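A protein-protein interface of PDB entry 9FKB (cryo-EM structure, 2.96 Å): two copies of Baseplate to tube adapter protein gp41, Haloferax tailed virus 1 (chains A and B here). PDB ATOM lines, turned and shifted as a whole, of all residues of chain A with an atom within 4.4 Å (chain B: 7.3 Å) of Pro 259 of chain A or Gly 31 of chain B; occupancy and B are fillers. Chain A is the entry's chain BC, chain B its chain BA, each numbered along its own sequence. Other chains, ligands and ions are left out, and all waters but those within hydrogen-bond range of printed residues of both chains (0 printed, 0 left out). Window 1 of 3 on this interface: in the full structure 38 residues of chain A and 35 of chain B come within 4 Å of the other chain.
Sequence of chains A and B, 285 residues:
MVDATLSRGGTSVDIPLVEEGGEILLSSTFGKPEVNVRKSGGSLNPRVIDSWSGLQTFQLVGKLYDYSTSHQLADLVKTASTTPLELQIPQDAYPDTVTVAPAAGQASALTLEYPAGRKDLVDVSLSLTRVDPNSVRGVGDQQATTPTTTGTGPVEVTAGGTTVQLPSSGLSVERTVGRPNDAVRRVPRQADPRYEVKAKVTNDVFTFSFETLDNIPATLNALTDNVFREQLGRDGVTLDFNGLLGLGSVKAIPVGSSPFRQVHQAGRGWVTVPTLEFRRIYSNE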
ATOM      1  N   PHE A 228      17.790  -4.988  16.428  1.00  0.00           N
ATOM      2  CA  PHE A 228      17.857  -6.203  15.615  1.00  0.00           C
ATOM      3  C   PHE A 228      17.168  -7.437  16.224  1.00  0.00           C
ATOM      4  O   PHE A 228      16.982  -8.425  15.504  1.00  0.00           O
ATOM      5  CB  PHE A 228      19.311  -6.513  15.240  1.00  0.00           C
ATOM      6  CG  PHE A 228      19.930  -5.479  14.331  1.00  0.00           C
ATOM      7  CD1 PHE A 228      19.674  -5.501  12.965  1.00  0.00           C
ATOM      8  CD2 PHE A 228      20.755  -4.471  14.829  1.00  0.00           C
ATOM      9  CE1 PHE A 228      20.233  -4.548  12.121  1.00  0.00           C
ATOM     10  CE2 PHE A 228      21.306  -3.505  13.989  1.00  0.00           C
ATOM     11  CZ  PHE A 228      21.009  -3.533  12.639  1.00  0.00           C
ATOM     12  N   PRO A 254      17.008  -0.511   9.778  1.00  0.00           N
ATOM     13  CA  PRO A 254      17.886  -1.368   8.977  1.00  0.00           C
ATOM     14  C   PRO A 254      17.168  -2.060   7.820  1.00  0.00           C
ATOM     15  O   PRO A 254      16.068  -2.575   7.989  1.00  0.00           O
ATOM     16  CB  PRO A 254      18.396  -2.421   9.977  1.00  0.00           C
ATOM     17  CG  PRO A 254      18.192  -1.790  11.334  1.00  0.00           C
ATOM     18  CD  PRO A 254      16.924  -0.982  11.167  1.00  0.00           C
ATOM     19  N   VAL A 255      17.804  -2.059   6.635  1.00  0.00           N
ATOM     20  CA  VAL A 255      17.264  -2.657   5.410  1.00  0.00           C
ATOM     21  C   VAL A 255      18.384  -3.375   4.645  1.00  0.00           C
ATOM     22  O   VAL A 255      19.528  -2.911   4.621  1.00  0.00           O
ATOM     23  CB  VAL A 255      16.525  -1.622   4.525  1.00  0.00           C
ATOM     24  CG1 VAL A 255      16.045  -2.198   3.190  1.00  0.00           C
ATOM     25  CG2 VAL A 255      15.348  -0.977   5.234  1.00  0.00           C
ATOM     26  N   GLY A 256      18.039  -4.506   4.000  1.00  0.00           N
ATOM     27  CA  GLY A 256      19.014  -5.432   3.434  1.00  0.00           C
ATOM     28  C   GLY A 256      19.358  -6.569   4.399  1.00  0.00           C
ATOM     29  O   GLY A 256      19.052  -6.506   5.589  1.00  0.00           O
ATOM     30  N   SER A 257      20.052  -7.597   3.884  1.00  0.00           N
ATOM     31  CA  SER A 257      20.210  -8.891   4.550  1.00  0.00           C
ATOM     32  C   SER A 257      21.103  -8.827   5.798  1.00  0.00           C
ATOM     33  O   SER A 257      20.899  -9.575   6.763  1.00  0.00           O
ATOM     34  CB  SER A 257      20.728  -9.925   3.580  1.00  0.00           C
ATOM     35  OG  SER A 257      19.898  -9.996   2.432  1.00  0.00           O
ATOM     36  N   SER A 258      22.111  -7.934   5.769  1.00  0.00           N
ATOM     37  CA  SER A 258      23.197  -7.857   6.750  1.00  0.00           C
ATOM     38  C   SER A 258      23.631  -6.403   7.008  1.00  0.00           C
ATOM     39  O   SER A 258      24.791  -6.063   6.772  1.00  0.00           O
ATOM     40  CB  SER A 258      24.372  -8.696   6.280  1.00  0.00           C
ATOM     41  OG  SER A 258      24.033 -10.073   6.166  1.00  0.00           O
ATOM     42  N   PRO A 259      22.746  -5.489   7.507  1.00  0.00           N
ATOM     43  CA  PRO A 259      23.075  -4.067   7.660  1.00  0.00           C
ATOM     44  C   PRO A 259      24.085  -3.783   8.769  1.00  0.00           C
ATOM     45  O   PRO A 259      24.744  -2.749   8.730  1.00  0.00           O
ATOM     46  CB  PRO A 259      21.736  -3.400   8.028  1.00  0.00           C
ATOM     47  CG  PRO A 259      20.684  -4.417   7.592  1.00  0.00           C
ATOM     48  CD  PRO A 259      21.357  -5.738   7.921  1.00  0.00           C
ATOM     49  N   PHE A 260      24.222  -4.709   9.729  1.00  0.00           N
ATOM     50  CA  PHE A 260      25.057  -4.475  10.894  1.00  0.00           C
ATOM     51  C   PHE A 260      25.987  -5.652  11.186  1.00  0.00           C
ATOM     52  O   PHE A 260      25.580  -6.812  11.130  1.00  0.00           O
ATOM     53  CB  PHE A 260      24.169  -4.150  12.084  1.00  0.00           C
ATOM     54  CG  PHE A 260      24.915  -4.092  13.390  1.00  0.00           C
ATOM     55  CD1 PHE A 260      25.628  -2.956  13.755  1.00  0.00           C
ATOM     56  CD2 PHE A 260      24.937  -5.192  14.239  1.00  0.00           C
ATOM     57  CE1 PHE A 260      26.293  -2.909  14.977  1.00  0.00           C
ATOM     58  CE2 PHE A 260      25.647  -5.161  15.432  1.00  0.00           C
ATOM     59  CZ  PHE A 260      26.308  -4.012  15.803  1.00  0.00           C
ATOM     60  N   THR A 275      30.015  -2.176   9.833  1.00  0.00           N
ATOM     61  CA  THR A 275      28.795  -1.569   9.318  1.00  0.00           C
ATOM     62  C   THR A 275      27.765  -1.408  10.429  1.00  0.00           C
ATOM     63  O   THR A 275      27.558  -2.303  11.250  1.00  0.00           O
ATOM     64  CB  THR A 275      28.147  -2.332   8.145  1.00  0.00           C
ATOM     65  OG1 THR A 275      27.575  -3.568   8.582  1.00  0.00           O
ATOM     66  CG2 THR A 275      29.067  -2.559   6.961  1.00  0.00           C
ATOM     67  N   LEU A 276      27.074  -0.270  10.368  1.00  0.00           N
ATOM     68  CA  LEU A 276      25.732  -0.087  10.882  1.00  0.00           C
ATOM     69  C   LEU A 276      24.997   0.739   9.824  1.00  0.00           C
ATOM     70  O   LEU A 276      25.246   1.934   9.669  1.00  0.00           O
ATOM     71  CB  LEU A 276      25.801   0.601  12.250  1.00  0.00           C
ATOM     72  CG  LEU A 276      24.461   1.032  12.848  1.00  0.00           C
ATOM     73  CD1 LEU A 276      23.526  -0.155  13.094  1.00  0.00           C
ATOM     74  CD2 LEU A 276      24.699   1.800  14.137  1.00  0.00           C
ATOM     75  N   GLU A 277      24.154   0.067   9.028  1.00  0.00           N
ATOM     76  CA  GLU A 277      23.433   0.698   7.930  1.00  0.00           C
ATOM     77  C   GLU A 277      21.966   0.923   8.312  1.00  0.00           C
ATOM     78  O   GLU A 277      21.297   0.013   8.801  1.00  0.00           O
ATOM     79  CB  GLU A 277      23.518  -0.169   6.672  1.00  0.00           C
ATOM     80  CG  GLU A 277      24.922  -0.378   6.119  1.00  0.00           C
ATOM     81  CD  GLU A 277      25.022  -1.543   5.142  1.00  0.00           C
ATOM     82  OE1 GLU A 277      23.999  -1.871   4.500  1.00  0.00           O
ATOM     83  OE2 GLU A 277      26.130  -2.124   5.020  1.00  0.00           O
ATOM     84  N   THR B  29      26.831 -11.014  12.663  1.00  0.00           N
ATOM     85  CA  THR B  29      26.122 -10.225  11.673  1.00  0.00           C
ATOM     86  C   THR B  29      24.644 -10.224  12.041  1.00  0.00           C
ATOM     87  O   THR B  29      24.092 -11.265  12.392  1.00  0.00           O
ATOM     88  CB  THR B  29      26.302 -10.826  10.272  1.00  0.00           C
ATOM     89  OG1 THR B  29      27.687 -10.877   9.936  1.00  0.00           O
ATOM     90  CG2 THR B  29      25.589 -10.061   9.179  1.00  0.00           C
ATOM     91  N   PHE B  30      24.010  -9.052  11.938  1.00  0.00           N
ATOM     92  CA  PHE B  30      22.575  -8.942  12.125  1.00  0.00           C
ATOM     93  C   PHE B  30      21.936  -8.288  10.907  1.00  0.00           C
ATOM     94  O   PHE B  30      22.558  -7.471  10.221  1.00  0.00           O
ATOM     95  CB  PHE B  30      22.265  -8.087  13.350  1.00  0.00           C
ATOM     96  CG  PHE B  30      22.731  -8.610  14.689  1.00  0.00           C
ATOM     97  CD1 PHE B  30      24.056  -8.477  15.106  1.00  0.00           C
ATOM     98  CD2 PHE B  30      21.832  -9.222  15.558  1.00  0.00           C
ATOM     99  CE1 PHE B  30      24.450  -8.892  16.375  1.00  0.00           C
ATOM    100  CE2 PHE B  30      22.222  -9.614  16.833  1.00  0.00           C
ATOM    101  CZ  PHE B  30      23.529  -9.444  17.242  1.00  0.00           C
ATOM    102  N   GLY B  31      20.661  -8.628  10.686  1.00  0.00           N
ATOM    103  CA  GLY B  31      19.837  -7.972   9.684  1.00  0.00           C
ATOM    104  C   GLY B  31      18.342  -8.234   9.866  1.00  0.00           C
ATOM    105  O   GLY B  31      17.952  -9.227  10.474  1.00  0.00           O
ATOM    106  N   LYS B  32      17.526  -7.350   9.272  1.00  0.00           N
ATOM    107  CA  LYS B  32      16.083  -7.500   9.159  1.00  0.00           C
ATOM    108  C   LYS B  32      15.721  -7.554   7.678  1.00  0.00           C
ATOM    109  O   LYS B  32      15.384  -6.540   7.069  1.00  0.00           O
ATOM    110  CB  LYS B  32      15.371  -6.373   9.911  1.00  0.00           C
ATOM    111  CG  LYS B  32      15.380  -6.545  11.423  1.00  0.00           C
ATOM    112  CD  LYS B  32      14.871  -5.342  12.159  1.00  0.00           C
ATOM    113  CE  LYS B  32      14.608  -5.612  13.629  1.00  0.00           C
ATOM    114  NZ  LYS B  32      13.382  -6.410  13.862  1.00  0.00           N
ATOM    115  N   PRO B  33      15.798  -8.749   7.044  1.00  0.00           N
ATOM    116  CA  PRO B  33      15.365  -8.891   5.655  1.00  0.00           C
ATOM    117  C   PRO B  33      13.852  -8.699   5.512  1.00  0.00           C
ATOM    118  O   PRO B  33      13.373  -8.310   4.456  1.00  0.00           O
ATOM    119  CB  PRO B  33      15.764 -10.331   5.276  1.00  0.00           C
ATOM    120  CG  PRO B  33      16.638 -10.853   6.419  1.00  0.00           C
ATOM    121  CD  PRO B  33      16.254 -10.025   7.627  1.00  0.00           C
ATOM    122  N   GLU B  34      13.105  -8.953   6.604  1.00  0.00           N
ATOM    123  CA  GLU B  34      11.661  -9.181   6.603  1.00  0.00           C
ATOM    124  C   GLU B  34      10.841  -7.953   7.055  1.00  0.00           C
ATOM    125  O   GLU B  34       9.659  -8.089   7.395  1.00  0.00           O
ATOM    126  CB  GLU B  34      11.349 -10.440   7.422  1.00  0.00           C
ATOM    127  CG  GLU B  34      12.134 -11.699   7.041  1.00  0.00           C
ATOM    128  CD  GLU B  34      12.025 -12.157   5.597  1.00  0.00           C
ATOM    129  OE1 GLU B  34      11.015 -11.802   4.943  1.00  0.00           O
ATOM    130  OE2 GLU B  34      12.909 -12.913   5.140  1.00  0.00           O
ATOM    131  N   SER B  53      10.624 -12.610  12.646  1.00  0.00           N
ATOM    132  CA  SER B  53      11.966 -13.021  13.048  1.00  0.00           C
ATOM    133  C   SER B  53      13.018 -12.496  12.066  1.00  0.00           C
ATOM    134  O   SER B  53      12.958 -12.819  10.882  1.00  0.00           O
ATOM    135  CB  SER B  53      12.034 -14.534  13.161  1.00  0.00           C
ATOM    136  OG  SER B  53      11.695 -15.111  11.915  1.00  0.00           O
ATOM    137  N   GLY B  54      13.994 -11.716  12.569  1.00  0.00           N
ATOM    138  CA  GLY B  54      15.123 -11.241  11.778  1.00  0.00           C
ATOM    139  C   GLY B  54      16.205 -12.310  11.600  1.00  0.00           C
ATOM    140  O   GLY B  54      15.950 -13.507  11.725  1.00  0.00           O
ATOM    141  N   LEU B  55      17.434 -11.868  11.334  1.00  0.00           N
ATOM    142  CA  LEU B  55      18.548 -12.773  11.111  1.00  0.00           C
ATOM    143  C   LEU B  55      19.729 -12.364  11.990  1.00  0.00           C
ATOM    144  O   LEU B  55      20.228 -11.249  11.862  1.00  0.00           O
ATOM    145  CB  LEU B  55      18.908 -12.717   9.621  1.00  0.00           C
ATOM    146  CG  LEU B  55      20.110 -13.542   9.171  1.00  0.00           C
ATOM    147  CD1 LEU B  55      19.987 -15.019   9.535  1.00  0.00           C
ATOM    148  CD2 LEU B  55      20.296 -13.386   7.674  1.00  0.00           C
ATOM    149  N   GLN B  56      20.191 -13.284  12.858  1.00  0.00           N
ATOM    150  CA  GLN B  56      21.517 -13.192  13.457  1.00  0.00           C
ATOM    151  C   GLN B  56      22.381 -14.368  12.990  1.00  0.00           C
ATOM    152  O   GLN B  56      21.934 -15.514  12.978  1.00  0.00           O
ATOM    153  CB  GLN B  56      21.456 -13.100  14.983  1.00  0.00           C
ATOM    154  CG  GLN B  56      22.850 -13.008  15.608  1.00  0.00           C
ATOM    155  CD  GLN B  56      22.866 -12.869  17.113  1.00  0.00           C
ATOM    156  OE1 GLN B  56      21.843 -13.024  17.782  1.00  0.00           O
ATOM    157  NE2 GLN B  56      24.025 -12.576  17.682  1.00  0.00           N
ATOM    158  N   THR B  57      23.631 -14.080  12.603  1.00  0.00           N
ATOM    159  CA  THR B  57      24.563 -15.089  12.115  1.00  0.00           C
ATOM    160  C   THR B  57      25.917 -14.925  12.806  1.00  0.00           C
ATOM    161  O   THR B  57      26.436 -13.812  12.851  1.00  0.00           O
ATOM    162  CB  THR B  57      24.793 -14.969  10.598  1.00  0.00           C
ATOM    163  OG1 THR B  57      23.568 -14.693   9.915  1.00  0.00           O
ATOM    164  CG2 THR B  57      25.418 -16.217  10.007  1.00  0.00           C
ATOM    165  N   ALA B 191      12.392 -12.882  17.871  1.00  0.00           N
ATOM    166  CA  ALA B 191      13.254 -12.446  16.776  1.00  0.00           C
ATOM    167  C   ALA B 191      14.032 -13.563  16.069  1.00  0.00           C
ATOM    168  O   ALA B 191      14.468 -13.344  14.944  1.00  0.00           O
ATOM    169  CB  ALA B 191      14.188 -11.367  17.238  1.00  0.00           C
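Of chain B, only Phe 30 (3.1 Å) and Gly 31 (3.2 Å) come within 4 Å of Pro 259 of chain A. Printed residues of chain A within 4 Å of Gly 31 of chain B: Phe 228, Ser 257 and Pro 259. Of the printed residues of chain B, Phe 228 of chain A touches Phe 30 (3.6 Å), Gly 31 (3.99 Å) and Lys 32 (3.9 Å). Of the printed residues of chain B, Ser 258 of chain A touches Thr 29 (3.4 Å) and Phe 30 (3.6 Å). Gly 54 of chain B touches none of the printed residues of chain A.
The backbone carbonyl oxygen (O) of Thr 57 of chain B sits at hydrogen-bond distance from the backbone NH (N) of Thr 29 of chain B (2.8 Å). The backbone NH (N) of Leu 55 of chain B sits at hydrogen-bond distance from the backbone carbonyl oxygen (O) of Gly 31 of chain B, 2.8 Å away. The side-chain hydroxyl of Thr 275 of chain A is in hydrogen-bond range of the backbone carbonyl oxygen of Pro 259 of chain A (3.0 Å). The backbone carbonyl oxygen (O) of Pro 259 of chain A lies within hydrogen-bond range of the backbone NH (N) of Glu 277 of chain A, 2.9 Å away.
The backbone carbonyl oxygen (O) of Phe 260 of chain A sits at hydrogen-bond distance from the backbone NH (N) of Phe 30 of chain B (2.9 Å). N of Pro 259 of chain A sits close to O of Phe 30 of chain B.
Phe 228 of chain A touches Phe 30 of chain B (CG to CB, 3.6 Å). Phe 228 of chain A touches Gly 31 of chain B. CE of Lys 32 of chain B touches CA of Phe 228 of chain A, 3.9 Å away. Gly 256 of chain A touches Lys 32 of chain B (O to O, 3.96 Å). Ser 257 of chain A touches Gly 31 of chain B. O of Ser 257 of chain A touches CD2 of Leu 55 of chain B, at 3.96 Å. Ser 258 of chain A touches Thr 29 of chain B. Ser 258 of chain A touches Phe 30 of chain B (CA to O, 3.6 Å). Pro 259 of chain A touches Gly 31 of chain B. Thr 29 of chain B touches Phe 260 of chain A (CA to O, 3.5 Å).
Of the 12 printed residues of chain B, 5 touch a printed residue of chain A. Hydrophobic or aromatic side chains of chain B that line the printed part of chain A: Phe 30 and Leu 55. Among the printed residues, 12 pairs touch across the chains. Among the printed residues, no Asp or Glu carboxylate lies within 4 Å of a Lys or Arg side-chain nitrogen of the other chain.
No position is printed for both chains.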
